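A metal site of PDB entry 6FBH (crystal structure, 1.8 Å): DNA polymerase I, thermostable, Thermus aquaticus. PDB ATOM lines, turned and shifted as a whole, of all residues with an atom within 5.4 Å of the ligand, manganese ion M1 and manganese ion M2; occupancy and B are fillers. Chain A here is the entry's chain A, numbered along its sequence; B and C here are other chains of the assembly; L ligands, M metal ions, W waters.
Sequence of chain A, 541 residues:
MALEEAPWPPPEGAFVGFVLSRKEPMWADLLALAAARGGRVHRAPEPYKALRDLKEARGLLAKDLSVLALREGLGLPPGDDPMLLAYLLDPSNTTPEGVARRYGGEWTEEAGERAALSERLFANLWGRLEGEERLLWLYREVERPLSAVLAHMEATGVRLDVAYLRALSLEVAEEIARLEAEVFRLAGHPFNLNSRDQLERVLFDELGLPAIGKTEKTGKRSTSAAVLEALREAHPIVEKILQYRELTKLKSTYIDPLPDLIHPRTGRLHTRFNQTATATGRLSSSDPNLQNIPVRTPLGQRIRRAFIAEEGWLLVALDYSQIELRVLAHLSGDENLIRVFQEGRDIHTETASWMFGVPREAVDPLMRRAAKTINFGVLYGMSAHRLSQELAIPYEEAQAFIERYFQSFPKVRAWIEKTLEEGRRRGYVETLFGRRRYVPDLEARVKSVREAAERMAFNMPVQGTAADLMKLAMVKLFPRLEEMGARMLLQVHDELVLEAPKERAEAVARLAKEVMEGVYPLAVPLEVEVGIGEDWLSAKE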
ATOM      1  N   ARG A 282      19.916  -7.639  13.191  1.00  0.00           N
ATOM      2  CA  ARG A 282      20.820  -8.765  12.967  1.00  0.00           C
ATOM      3  C   ARG A 282      20.612  -9.371  11.586  1.00  0.00           C
ATOM      4  O   ARG A 282      19.527  -9.296  11.001  1.00  0.00           O
ATOM      5  CB  ARG A 282      20.598  -9.843  14.026  1.00  0.00           C
ATOM      6  CG  ARG A 282      21.269  -9.586  15.335  1.00  0.00           C
ATOM      7  CD  ARG A 282      21.109 -10.772  16.217  1.00  0.00           C
ATOM      8  NE  ARG A 282      22.013 -10.772  17.343  1.00  0.00           N
ATOM      9  CZ  ARG A 282      22.237 -11.825  18.108  1.00  0.00           C
ATOM     10  NH1 ARG A 282      21.594 -12.974  17.872  1.00  0.00           N
ATOM     11  NH2 ARG A 282      23.110 -11.741  19.107  1.00  0.00           N
ATOM     12  N   ASP A 319      36.076 -11.730  17.488  1.00  0.00           N
ATOM     13  CA  ASP A 319      34.836 -11.764  18.247  1.00  0.00           C
ATOM     14  C   ASP A 319      34.875 -10.659  19.287  1.00  0.00           C
ATOM     15  O   ASP A 319      35.757 -10.655  20.155  1.00  0.00           O
ATOM     16  CB  ASP A 319      34.641 -13.137  18.883  1.00  0.00           C
ATOM     17  CG  ASP A 319      33.303 -13.252  19.615  1.00  0.00           C
ATOM     18  OD1 ASP A 319      33.098 -12.485  20.570  1.00  0.00           O
ATOM     19  OD2 ASP A 319      32.490 -14.094  19.205  1.00  0.00           O
ATOM     20  N   TYR A 320      33.935  -9.718  19.200  1.00  0.00           N
ATOM     21  CA  TYR A 320      33.848  -8.639  20.174  1.00  0.00           C
ATOM     22  C   TYR A 320      33.684  -9.193  21.579  1.00  0.00           C
ATOM     23  O   TYR A 320      32.960 -10.169  21.819  1.00  0.00           O
ATOM     24  CB  TYR A 320      32.675  -7.725  19.855  1.00  0.00           C
ATOM     25  CG  TYR A 320      32.860  -6.797  18.675  1.00  0.00           C
ATOM     26  CD1 TYR A 320      33.671  -5.670  18.779  1.00  0.00           C
ATOM     27  CD2 TYR A 320      32.209  -7.020  17.478  1.00  0.00           C
ATOM     28  CE1 TYR A 320      33.841  -4.797  17.697  1.00  0.00           C
ATOM     29  CE2 TYR A 320      32.360  -6.173  16.406  1.00  0.00           C
ATOM     30  CZ  TYR A 320      33.176  -5.070  16.517  1.00  0.00           C
ATOM     31  OH  TYR A 320      33.327  -4.223  15.445  1.00  0.00           O
ATOM     32  N   SER A 321      34.368  -8.552  22.527  1.00  0.00           N
ATOM     33  CA  SER A 321      34.288  -8.920  23.927  1.00  0.00           C
ATOM     34  C   SER A 321      33.025  -8.339  24.555  1.00  0.00           C
ATOM     35  O   SER A 321      32.760  -7.139  24.422  1.00  0.00           O
ATOM     36  CB  SER A 321      35.543  -8.426  24.652  1.00  0.00           C
ATOM     37  OG  SER A 321      35.478  -8.698  26.037  1.00  0.00           O
ATOM     38  N   GLN A 322      32.241  -9.203  25.202  1.00  0.00           N
ATOM     39  CA  GLN A 322      31.104  -8.789  26.065  1.00  0.00           C
ATOM     40  C   GLN A 322      30.263  -7.702  25.399  1.00  0.00           C
ATOM     41  O   GLN A 322      29.954  -6.663  25.993  1.00  0.00           O
ATOM     42  CB  GLN A 322      31.603  -8.292  27.421  1.00  0.00           C
ATOM     43  CG  GLN A 322      32.584  -9.209  28.140  1.00  0.00           C
ATOM     44  CD  GLN A 322      33.176  -8.564  29.379  1.00  0.00           C
ATOM     45  OE1 GLN A 322      32.538  -8.504  30.427  1.00  0.00           O
ATOM     46  NE2 GLN A 322      34.408  -8.071  29.258  1.00  0.00           N
ATOM     47  N   ILE A 323      29.887  -7.947  24.147  1.00  0.00           N
ATOM     48  CA  ILE A 323      29.536  -6.831  23.268  1.00  0.00           C
ATOM     49  C   ILE A 323      28.277  -6.125  23.757  1.00  0.00           C
ATOM     50  O   ILE A 323      28.260  -4.893  23.865  1.00  0.00           O
ATOM     51  CB  ILE A 323      29.411  -7.308  21.799  1.00  0.00           C
ATOM     52  CG1 ILE A 323      29.106  -6.119  20.895  1.00  0.00           C
ATOM     53  CG2 ILE A 323      28.324  -8.364  21.620  1.00  0.00           C
ATOM     54  CD1 ILE A 323      30.152  -5.051  20.902  1.00  0.00           C
ATOM     55  N   GLU A 324      27.195  -6.864  24.032  1.00  0.00           N
ATOM     56  CA  GLU A 324      25.971  -6.165  24.419  1.00  0.00           C
ATOM     57  C   GLU A 324      26.134  -5.478  25.779  1.00  0.00           C
ATOM     58  O   GLU A 324      25.486  -4.458  26.032  1.00  0.00           O
ATOM     59  CB  GLU A 324      24.756  -7.121  24.382  1.00  0.00           C
ATOM     60  CG  GLU A 324      24.210  -7.305  22.960  1.00  0.00           C
ATOM     61  CD  GLU A 324      22.990  -8.201  22.862  1.00  0.00           C
ATOM     62  OE1 GLU A 324      22.178  -8.193  23.805  1.00  0.00           O
ATOM     63  OE2 GLU A 324      22.849  -8.939  21.848  1.00  0.00           O
ATOM     64  N   LEU A 325      27.027  -5.980  26.640  1.00  0.00           N
ATOM     65  CA  LEU A 325      27.280  -5.260  27.899  1.00  0.00           C
ATOM     66  C   LEU A 325      28.031  -3.955  27.649  1.00  0.00           C
ATOM     67  O   LEU A 325      27.748  -2.939  28.310  1.00  0.00           O
ATOM     68  CB  LEU A 325      28.044  -6.149  28.893  1.00  0.00           C
ATOM     69  CG  LEU A 325      27.271  -7.367  29.436  1.00  0.00           C
ATOM     70  CD1 LEU A 325      28.093  -8.156  30.471  1.00  0.00           C
ATOM     71  CD2 LEU A 325      25.937  -6.928  30.046  1.00  0.00           C
ATOM     72  N   ASP A 346      35.961  -8.516  33.380  1.00  0.00           N
ATOM     73  CA  ASP A 346      35.176  -9.453  32.592  1.00  0.00           C
ATOM     74  C   ASP A 346      34.013  -9.930  33.451  1.00  0.00           C
ATOM     75  O   ASP A 346      34.209 -10.697  34.403  1.00  0.00           O
ATOM     76  CB  ASP A 346      36.027 -10.640  32.127  1.00  0.00           C
ATOM     77  CG  ASP A 346      35.283 -11.543  31.152  1.00  0.00           C
ATOM     78  OD1 ASP A 346      34.051 -11.702  31.288  1.00  0.00           O
ATOM     79  OD2 ASP A 346      35.928 -12.087  30.222  1.00  0.00           O
ATOM     80  N   HIS A 348      31.473 -11.852  32.573  1.00  0.00           N
ATOM     81  CA  HIS A 348      31.183 -13.272  32.396  1.00  0.00           C
ATOM     82  C   HIS A 348      32.074 -14.122  33.291  1.00  0.00           C
ATOM     83  O   HIS A 348      31.613 -15.069  33.927  1.00  0.00           O
ATOM     84  CB  HIS A 348      31.347 -13.676  30.922  1.00  0.00           C
ATOM     85  CG  HIS A 348      30.416 -12.951  29.991  1.00  0.00           C
ATOM     86  ND1 HIS A 348      29.142 -12.585  30.343  1.00  0.00           N
ATOM     87  CD2 HIS A 348      30.597 -12.525  28.713  1.00  0.00           C
ATOM     88  CE1 HIS A 348      28.558 -11.976  29.320  1.00  0.00           C
ATOM     89  NE2 HIS A 348      29.428 -11.921  28.320  1.00  0.00           N
ATOM     90  N   ARG A 368      32.240 -20.320  31.611  1.00  0.00           N
ATOM     91  CA  ARG A 368      32.030 -18.942  31.188  1.00  0.00           C
ATOM     92  C   ARG A 368      30.765 -18.823  30.333  1.00  0.00           C
ATOM     93  O   ARG A 368      30.017 -17.850  30.455  1.00  0.00           O
ATOM     94  CB  ARG A 368      33.261 -18.439  30.428  1.00  0.00           C
ATOM     95  CG  ARG A 368      33.364 -16.929  30.324  1.00  0.00           C
ATOM     96  CD  ARG A 368      34.728 -16.443  29.781  1.00  0.00           C
ATOM     97  NE  ARG A 368      34.707 -14.997  29.576  1.00  0.00           N
ATOM     98  CZ  ARG A 368      34.142 -14.404  28.525  1.00  0.00           C
ATOM     99  NH1 ARG A 368      33.560 -15.130  27.582  1.00  0.00           N
ATOM    100  NH2 ARG A 368      34.151 -13.091  28.423  1.00  0.00           N
ATOM    101  N   ARG A 369      30.514 -19.821  29.477  1.00  0.00           N
ATOM    102  CA  ARG A 369      29.291 -19.810  28.677  1.00  0.00           C
ATOM    103  C   ARG A 369      28.061 -19.829  29.577  1.00  0.00           C
ATOM    104  O   ARG A 369      27.100 -19.081  29.352  1.00  0.00           O
ATOM    105  CB  ARG A 369      29.289 -21.008  27.720  1.00  0.00           C
ATOM    106  CG  ARG A 369      28.669 -20.733  26.351  1.00  0.00           C
ATOM    107  CD  ARG A 369      27.177 -20.384  26.421  1.00  0.00           C
ATOM    108  NE  ARG A 369      26.846 -19.227  25.572  1.00  0.00           N
ATOM    109  CZ  ARG A 369      25.748 -18.488  25.705  1.00  0.00           C
ATOM    110  NH1 ARG A 369      24.862 -18.742  26.661  1.00  0.00           N
ATOM    111  NH2 ARG A 369      25.534 -17.464  24.884  1.00  0.00           N
ATOM    112  N   LYS A 372      27.590 -16.534  30.918  1.00  0.00           N
ATOM    113  CA  LYS A 372      27.070 -15.685  29.863  1.00  0.00           C
ATOM    114  C   LYS A 372      25.536 -15.716  29.843  1.00  0.00           C
ATOM    115  O   LYS A 372      24.868 -14.677  29.812  1.00  0.00           O
ATOM    116  CB  LYS A 372      27.645 -16.170  28.533  1.00  0.00           C
ATOM    117  CG  LYS A 372      27.480 -15.245  27.387  1.00  0.00           C
ATOM    118  CD  LYS A 372      28.237 -15.801  26.194  1.00  0.00           C
ATOM    119  CE  LYS A 372      29.765 -15.624  26.368  1.00  0.00           C
ATOM    120  NZ  LYS A 372      30.510 -16.124  25.185  1.00  0.00           N
ATOM    121  N   THR A 373      24.956 -16.921  29.864  1.00  0.00           N
ATOM    122  CA  THR A 373      23.502 -17.036  29.811  1.00  0.00           C
ATOM    123  C   THR A 373      22.850 -16.395  31.026  1.00  0.00           C
ATOM    124  O   THR A 373      21.777 -15.776  30.904  1.00  0.00           O
ATOM    125  CB  THR A 373      23.132 -18.508  29.712  1.00  0.00           C
ATOM    126  OG1 THR A 373      23.937 -19.134  28.712  1.00  0.00           O
ATOM    127  CG2 THR A 373      21.663 -18.670  29.364  1.00  0.00           C
ATOM    128  N   PHE A 376      22.984 -12.364  30.634  1.00  0.00           N
ATOM    129  CA  PHE A 376      22.007 -11.806  29.726  1.00  0.00           C
ATOM    130  C   PHE A 376      20.600 -12.237  30.115  1.00  0.00           C
ATOM    131  O   PHE A 376      19.667 -11.445  30.005  1.00  0.00           O
ATOM    132  CB  PHE A 376      22.375 -12.186  28.273  1.00  0.00           C
ATOM    133  CG  PHE A 376      23.616 -11.478  27.798  1.00  0.00           C
ATOM    134  CD1 PHE A 376      23.627 -10.107  27.688  1.00  0.00           C
ATOM    135  CD2 PHE A 376      24.792 -12.170  27.514  1.00  0.00           C
ATOM    136  CE1 PHE A 376      24.771  -9.427  27.286  1.00  0.00           C
ATOM    137  CE2 PHE A 376      25.935 -11.496  27.104  1.00  0.00           C
ATOM    138  CZ  PHE A 376      25.917 -10.126  26.986  1.00  0.00           C
ATOM    139  N   GLY A 377      20.443 -13.443  30.625  1.00  0.00           N
ATOM    140  CA  GLY A 377      19.127 -13.841  31.118  1.00  0.00           C
ATOM    141  C   GLY A 377      18.592 -12.845  32.123  1.00  0.00           C
ATOM    142  O   GLY A 377      17.471 -12.354  31.995  1.00  0.00           O
ATOM    143  N   TYR A 380      17.818  -9.128  30.626  1.00  0.00           N
ATOM    144  CA  TYR A 380      16.653  -8.971  29.779  1.00  0.00           C
ATOM    145  C   TYR A 380      15.391  -9.537  30.400  1.00  0.00           C
ATOM    146  O   TYR A 380      14.390  -9.717  29.688  1.00  0.00           O
ATOM    147  CB  TYR A 380      16.923  -9.629  28.419  1.00  0.00           C
ATOM    148  CG  TYR A 380      18.000  -8.910  27.647  1.00  0.00           C
ATOM    149  CD1 TYR A 380      17.878  -7.561  27.352  1.00  0.00           C
ATOM    150  CD2 TYR A 380      19.144  -9.573  27.201  1.00  0.00           C
ATOM    151  CE1 TYR A 380      18.864  -6.885  26.624  1.00  0.00           C
ATOM    152  CE2 TYR A 380      20.136  -8.897  26.486  1.00  0.00           C
ATOM    153  CZ  TYR A 380      19.986  -7.547  26.208  1.00  0.00           C
ATOM    154  OH  TYR A 380      20.951  -6.867  25.493  1.00  0.00           O
ATOM    155  N   ASN A 459      15.291  -5.008  24.705  1.00  0.00           N
ATOM    156  CA  ASN A 459      16.391  -5.778  24.120  1.00  0.00           C
ATOM    157  C   ASN A 459      16.842  -5.168  22.802  1.00  0.00           C
ATOM    158  O   ASN A 459      18.055  -5.085  22.536  1.00  0.00           O
ATOM    159  CB  ASN A 459      15.959  -7.230  23.934  1.00  0.00           C
ATOM    160  CG  ASN A 459      16.956  -8.064  23.129  1.00  0.00           C
ATOM    161  OD1 ASN A 459      16.816  -8.213  21.913  1.00  0.00           O
ATOM    162  ND2 ASN A 459      17.934  -8.662  23.798  1.00  0.00           N
ATOM    163  N   VAL A 492      28.987 -14.214  12.452  1.00  0.00           N
ATOM    164  CA  VAL A 492      28.168 -14.879  13.459  1.00  0.00           C
ATOM    165  C   VAL A 492      27.788 -13.850  14.522  1.00  0.00           C
ATOM    166  O   VAL A 492      28.150 -13.984  15.692  1.00  0.00           O
ATOM    167  CB  VAL A 492      28.905 -16.088  14.069  1.00  0.00           C
ATOM    168  CG1 VAL A 492      27.952 -16.935  14.865  1.00  0.00           C
ATOM    169  CG2 VAL A 492      29.543 -16.919  12.958  1.00  0.00           C
ATOM    170  N   ASP A 494      28.497 -11.234  16.290  1.00  0.00           N
ATOM    171  CA  ASP A 494      29.534 -10.326  16.774  1.00  0.00           C
ATOM    172  C   ASP A 494      30.924 -10.877  16.441  1.00  0.00           C
ATOM    173  O   ASP A 494      31.910 -10.506  17.092  1.00  0.00           O
ATOM    174  CB  ASP A 494      29.396 -10.035  18.271  1.00  0.00           C
ATOM    175  CG  ASP A 494      29.911 -11.153  19.143  1.00  0.00           C
ATOM    176  OD1 ASP A 494      29.767 -12.306  18.721  1.00  0.00           O
ATOM    177  OD2 ASP A 494      30.444 -10.860  20.247  1.00  0.00           O
ATOM    178  N   GLU A 495      31.003 -11.722  15.436  1.00  0.00           N
ATOM    179  CA  GLU A 495      32.208 -12.457  15.092  1.00  0.00           C
ATOM    180  C   GLU A 495      32.344 -12.479  13.586  1.00  0.00           C
ATOM    181  O   GLU A 495      31.340 -12.530  12.861  1.00  0.00           O
ATOM    182  CB  GLU A 495      32.160 -13.892  15.657  1.00  0.00           C
ATOM    183  CG  GLU A 495      33.233 -14.838  15.100  1.00  0.00           C
ATOM    184  CD  GLU A 495      33.080 -16.261  15.604  1.00  0.00           C
ATOM    185  OE1 GLU A 495      32.139 -16.500  16.413  1.00  0.00           O
ATOM    186  OE2 GLU A 495      33.886 -17.128  15.196  1.00  0.00           O
ATOM    187  N   LYS A 540      39.505 -19.859  17.359  1.00  0.00           N
ATOM    188  CA  LYS A 540      38.813 -19.197  18.458  1.00  0.00           C
ATOM    189  C   LYS A 540      39.513 -19.369  19.798  1.00  0.00           C
ATOM    190  O   LYS A 540      38.897 -19.108  20.836  1.00  0.00           O
ATOM    191  CB  LYS A 540      37.369 -19.683  18.573  1.00  0.00           C
ATOM    192  CG  LYS A 540      36.458 -19.245  17.418  1.00  0.00           C
ATOM    193  CD  LYS A 540      35.037 -18.955  17.887  1.00  0.00           C
ATOM    194  CE  LYS A 540      34.966 -17.619  18.627  1.00  0.00           C
ATOM    195  NZ  LYS A 540      33.585 -17.256  19.059  1.00  0.00           N
ATOM    196  P    DC B  12      28.319 -19.457  19.845  1.00  0.00           P
ATOM    197  OP1  DC B  12      29.721 -19.303  19.396  1.00  0.00           O
ATOM    198  OP2  DC B  12      27.985 -19.900  21.220  1.00  0.00           O
ATOM    199  O5'  DC B  12      27.546 -18.070  19.612  1.00  0.00           O
ATOM    200  C5'  DC B  12      27.673 -17.385  18.339  1.00  0.00           C
ATOM    201  C4'  DC B  12      26.814 -16.142  18.309  1.00  0.00           C
ATOM    202  O4'  DC B  12      25.428 -16.523  18.449  1.00  0.00           O
ATOM    203  C3'  DC B  12      27.075 -15.179  19.462  1.00  0.00           C
ATOM    204  O3'  DC B  12      28.008 -14.236  19.107  1.00  0.00           O
ATOM    205  C2'  DC B  12      25.721 -14.528  19.711  1.00  0.00           C
ATOM    206  C1'  DC B  12      24.725 -15.544  19.192  1.00  0.00           C
ATOM    207  N1   DC B  12      23.967 -16.238  20.253  1.00  0.00           N
ATOM    208  C2   DC B  12      22.733 -15.743  20.625  1.00  0.00           C
ATOM    209  O2   DC B  12      22.337 -14.696  20.091  1.00  0.00           O
ATOM    210  N3   DC B  12      22.018 -16.385  21.588  1.00  0.00           N
ATOM    211  C4   DC B  12      22.497 -17.502  22.130  1.00  0.00           C
ATOM    212  N4   DC B  12      21.759 -18.107  23.066  1.00  0.00           N
ATOM    213  C5   DC B  12      23.752 -18.041  21.752  1.00  0.00           C
ATOM    214  C6   DC B  12      24.456 -17.378  20.813  1.00  0.00           C
ATOM    215  P    DC C   4      11.651 -16.296  32.005  1.00  0.00           P
ATOM    216  OP1  DC C   4      11.608 -17.631  31.381  1.00  0.00           O
ATOM    217  OP2  DC C   4      11.774 -16.164  33.468  1.00  0.00           O
ATOM    218  O5'  DC C   4      12.859 -15.466  31.371  1.00  0.00           O
ATOM    219  C5'  DC C   4      12.891 -15.277  29.980  1.00  0.00           C
ATOM    220  C4'  DC C   4      13.563 -13.973  29.637  1.00  0.00           C
ATOM    221  O4'  DC C   4      14.927 -13.991  30.116  1.00  0.00           O
ATOM    222  C3'  DC C   4      13.643 -13.693  28.153  1.00  0.00           C
ATOM    223  O3'  DC C   4      12.506 -13.020  27.726  1.00  0.00           O
ATOM    224  C2'  DC C   4      14.914 -12.841  28.049  1.00  0.00           C
ATOM    225  C1'  DC C   4      15.791 -13.449  29.137  1.00  0.00           C
ATOM    226  N1   DC C   4      16.696 -14.518  28.635  1.00  0.00           N
ATOM    227  C2   DC C   4      17.750 -14.146  27.796  1.00  0.00           C
ATOM    228  O2   DC C   4      17.869 -12.960  27.512  1.00  0.00           O
ATOM    229  N3   DC C   4      18.603 -15.086  27.351  1.00  0.00           N
ATOM    230  C4   DC C   4      18.444 -16.350  27.690  1.00  0.00           C
ATOM    231  N4   DC C   4      19.318 -17.243  27.218  1.00  0.00           N
ATOM    232  C5   DC C   4      17.347 -16.774  28.537  1.00  0.00           C
ATOM    233  C6   DC C   4      16.517 -15.825  28.985  1.00  0.00           C
ATOM    234  P    DG C   5      11.780 -13.448  26.356  1.00  0.00           P
ATOM    235  OP1  DG C   5      10.514 -12.686  26.375  1.00  0.00           O
ATOM    236  OP2  DG C   5      11.834 -14.914  26.172  1.00  0.00           O
ATOM    237  O5'  DG C   5      12.692 -12.825  25.203  1.00  0.00           O
ATOM    238  C5'  DG C   5      12.685 -11.428  24.997  1.00  0.00           C
ATOM    239  C4'  DG C   5      13.841 -10.997  24.124  1.00  0.00           C
ATOM    240  O4'  DG C   5      15.083 -11.452  24.723  1.00  0.00           O
ATOM    241  C3'  DG C   5      13.867 -11.563  22.721  1.00  0.00           C
ATOM    242  O3'  DG C   5      13.059 -10.783  21.833  1.00  0.00           O
ATOM    243  C2'  DG C   5      15.351 -11.480  22.369  1.00  0.00           C
ATOM    244  C1'  DG C   5      16.025 -11.736  23.716  1.00  0.00           C
ATOM    245  N9   DG C   5      16.485 -13.109  23.885  1.00  0.00           N
ATOM    246  C8   DG C   5      15.950 -14.080  24.704  1.00  0.00           C
ATOM    247  N7   DG C   5      16.611 -15.209  24.680  1.00  0.00           N
ATOM    248  C5   DG C   5      17.648 -14.951  23.766  1.00  0.00           C
ATOM    249  C6   DG C   5      18.694 -15.792  23.309  1.00  0.00           C
ATOM    250  O6   DG C   5      18.943 -16.961  23.624  1.00  0.00           O
ATOM    251  N1   DG C   5      19.526 -15.134  22.409  1.00  0.00           N
ATOM    252  C2   DG C   5      19.361 -13.833  21.990  1.00  0.00           C
ATOM    253  N2   DG C   5      20.257 -13.365  21.106  1.00  0.00           N
ATOM    254  N3   DG C   5      18.394 -13.036  22.409  1.00  0.00           N
ATOM    255  C4   DG C   5      17.573 -13.668  23.287  1.00  0.00           C
HETATM  256  N1  LIG L   1      20.744 -14.404  25.693  1.00  0.00           N
HETATM  257  C1  LIG L   1      20.654 -13.172  25.114  1.00  0.00           C
HETATM  258  N2  LIG L   1      19.576 -12.449  25.400  1.00  0.00           N
HETATM  259  N3  LIG L   1      21.585 -12.669  24.301  1.00  0.00           N
HETATM  260  C2  LIG L   1      22.617 -13.514  24.106  1.00  0.00           C
HETATM  261  C3  LIG L   1      22.781 -14.774  24.607  1.00  0.00           C
HETATM  262  C4  LIG L   1      21.768 -15.301  25.501  1.00  0.00           C
HETATM  263  O1  LIG L   1      21.774 -16.380  26.083  1.00  0.00           O
HETATM  264  N4  LIG L   1      23.961 -15.338  24.143  1.00  0.00           N
HETATM  265  C5  LIG L   1      24.476 -14.413  23.376  1.00  0.00           C
HETATM  266  N5  LIG L   1      23.723 -13.274  23.340  1.00  0.00           N
HETATM  267  P1  LIG L   1      29.010 -13.955  22.468  1.00  0.00           P
HETATM  268  P2  LIG L   1      29.886 -11.991  24.468  1.00  0.00           P
HETATM  269  P3  LIG L   1      32.569 -12.901  24.871  1.00  0.00           P
HETATM  270  C6  LIG L   1      24.100 -11.976  22.768  1.00  0.00           C
HETATM  271  O2  LIG L   1      30.025 -13.550  21.504  1.00  0.00           O
HETATM  272  O3  LIG L   1      30.122 -11.058  23.382  1.00  0.00           O
HETATM  273  O4  LIG L   1      33.598 -12.148  25.635  1.00  0.00           O
HETATM  274  C7  LIG L   1      24.728 -11.046  23.812  1.00  0.00           C
HETATM  275  O5  LIG L   1      28.932 -15.486  22.483  1.00  0.00           O
HETATM  276  O6  LIG L   1      28.865 -11.232  25.401  1.00  0.00           O
HETATM  277  O7  LIG L   1      32.690 -14.396  25.090  1.00  0.00           O
HETATM  278  C8  LIG L   1      26.231 -11.175  23.552  1.00  0.00           C
HETATM  279  O8  LIG L   1      26.892  -9.959  23.886  1.00  0.00           O
HETATM  280  N6  LIG L   1      29.336 -13.423  23.959  1.00  0.00           N
HETATM  281  O9  LIG L   1      31.146 -12.381  25.362  1.00  0.00           O
HETATM  282  O10 LIG L   1      32.540 -12.631  23.344  1.00  0.00           O
HETATM  283  C9  LIG L   1      26.264 -11.405  22.045  1.00  0.00           C
HETATM  284  O11 LIG L   1      25.093 -12.202  21.772  1.00  0.00           O
HETATM  285  C10 LIG L   1      27.492 -12.079  21.509  1.00  0.00           C
HETATM  286  O12 LIG L   1      27.604 -13.398  22.064  1.00  0.00           O
HETATM  287 MN    MN M   1      31.497 -11.787  21.841  1.00  0.00          MN
HETATM  288 MN    MN M   2      30.308 -14.157  19.457  1.00  0.00          MN
HETATM  289  O   HOH W   1      30.238 -15.365  17.770  1.00  0.00           O
HETATM  290  O   HOH W   2      35.283 -12.587  22.484  1.00  0.00           O
HETATM  291  O   HOH W   3      24.484  -9.395  19.800  1.00  0.00           O
HETATM  292  O   HOH W   4      20.456 -10.242  22.929  1.00  0.00           O
HETATM  293  O   HOH W   5      30.591 -15.774  20.218  1.00  0.00           O
HETATM  294  O   HOH W   6      27.461 -17.928  22.935  1.00  0.00           O
HETATM  295  O   HOH W   7      32.663 -15.533  22.206  1.00  0.00           O
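Manganese ion M2 is bound by water W5, the side-chain carboxylate (OD1) of Asp 494, water W1, an oxygen (O2) of the ligand, the side-chain carboxylate (OD2) of Asp 319 and O3' of DC 12 of chain B.
OD2 of Asp 319 sits close to NZ of Lys 540. OD1 of Asp 346 is in hydrogen-bond range of N of His 348. The side-chain amide nitrogen of Gln 322 sits at hydrogen-bond distance from the side-chain hydroxyl of Ser 321 (3.5 Å). O2 of DC 12 of chain B is in hydrogen-bond range of the guanidinium group of Arg 282. The side-chain carboxylate (OE2) of Glu 324 is in salt-bridge range of the guanidinium group (NH2) of Arg 282, at 3.9 Å. The guanidinium group (NH2) of Arg 368 lies within salt-bridge range of the side-chain carboxylate (OD2) of Asp 346 (2.7 Å). The side-chain carboxylate (OE1) of Glu 324 sits at hydrogen-bond distance from the side-chain hydroxyl (OH) of Tyr 380 (2.5 Å). OG1 of Thr 373 is in hydrogen-bond range of O of Arg 369.
O2 of DC 4 of chain C lies within hydrogen-bond range of a nitrogen (N2) of the ligand. N of Ile 323 lies close to O3 of the ligand. The guanidinium group (NH2) of Arg 282 is in hydrogen-bond range of an oxygen (O11) of the ligand, at 3.4 Å. N4 of the ligand sits at hydrogen-bond distance from NH2 of Arg 369 (2.7 Å). The backbone NH of Gln 322 lies within hydrogen-bond range of an oxygen (O4) of the ligand. A ring nitrogen (NE2) of His 348 sits at hydrogen-bond distance from an oxygen (O6) of the ligand (3.1 Å). N of Glu 324 lies within hydrogen-bond range of O8 of the ligand, 3.1 Å away. The side-chain amino group (NZ) of Lys 372 lies within salt-bridge range of an oxygen (O7) of the ligand (2.8 Å). NH1 of Arg 368 lies within salt-bridge range of O7 of the ligand, 2.7 Å away. N3 of DG 5 of chain C lies close to N2 of the ligand (3.3 Å).
The nearest printed residue that does not touch manganese ion M2 is Glu 495 (4.2 Å).
Manganese ion M1 is bound by O10 of the ligand (2.0 Å). Manganese ion M1 is bound by OD2 of Asp 494, at 2.1 Å. The side-chain carboxylate (OD1) of Asp 319 is bound to manganese ion M1, at 2.2 Å. O of Tyr 320 binds manganese ion M1 (2.2 Å). Manganese ion M1 is bound by O3 of the ligand, 2.2 Å away. An oxygen (O2) of the ligand is bound to manganese ion M1, 2.3 Å away.
Residues that only touch the ligand: Phe 376, Tyr 380 and Ser 321. Hydrophobic or aromatic side chains that line the ligand: Ile 323, His 348, Phe 376 and Tyr 380. 17 residues have an atom within 4 Å of the ligand: Arg 282, Asp 319, Tyr 320, Ser 321, Gln 322, Ile 323, Glu 324, His 348, Arg 368, Arg 369, Lys 372, Phe 376, Tyr 380, Asp 494, DC 12 of chain B, DC 4 of chain C and DG 5 of chain C.
Of the 25 residues printed, 3 come within 4 Å of manganese ion M1.
Water W1 bridges OE1 of Glu 495 (2.6 Å) and O of Val 492 (3.3 Å). Water W6 lies within hydrogen-bond range of OP2 of DC 12 of chain B (2.7 Å), the guanidinium group of Arg 369 (2.8 Å) and an oxygen (O5) of the ligand (2.9 Å). Water W4 lies within hydrogen-bond range of the side-chain carboxylate of Glu 324 (2.8 Å), a nitrogen (N3) of the ligand (3.0 Å) and the side-chain amide nitrogen of Asn 459 (3.1 Å). Water W3 lies within hydrogen-bond range of OE2 of Glu 324 (2.7 Å), NH2 of Arg 282 (2.8 Å) and O11 of the ligand (3.5 Å).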
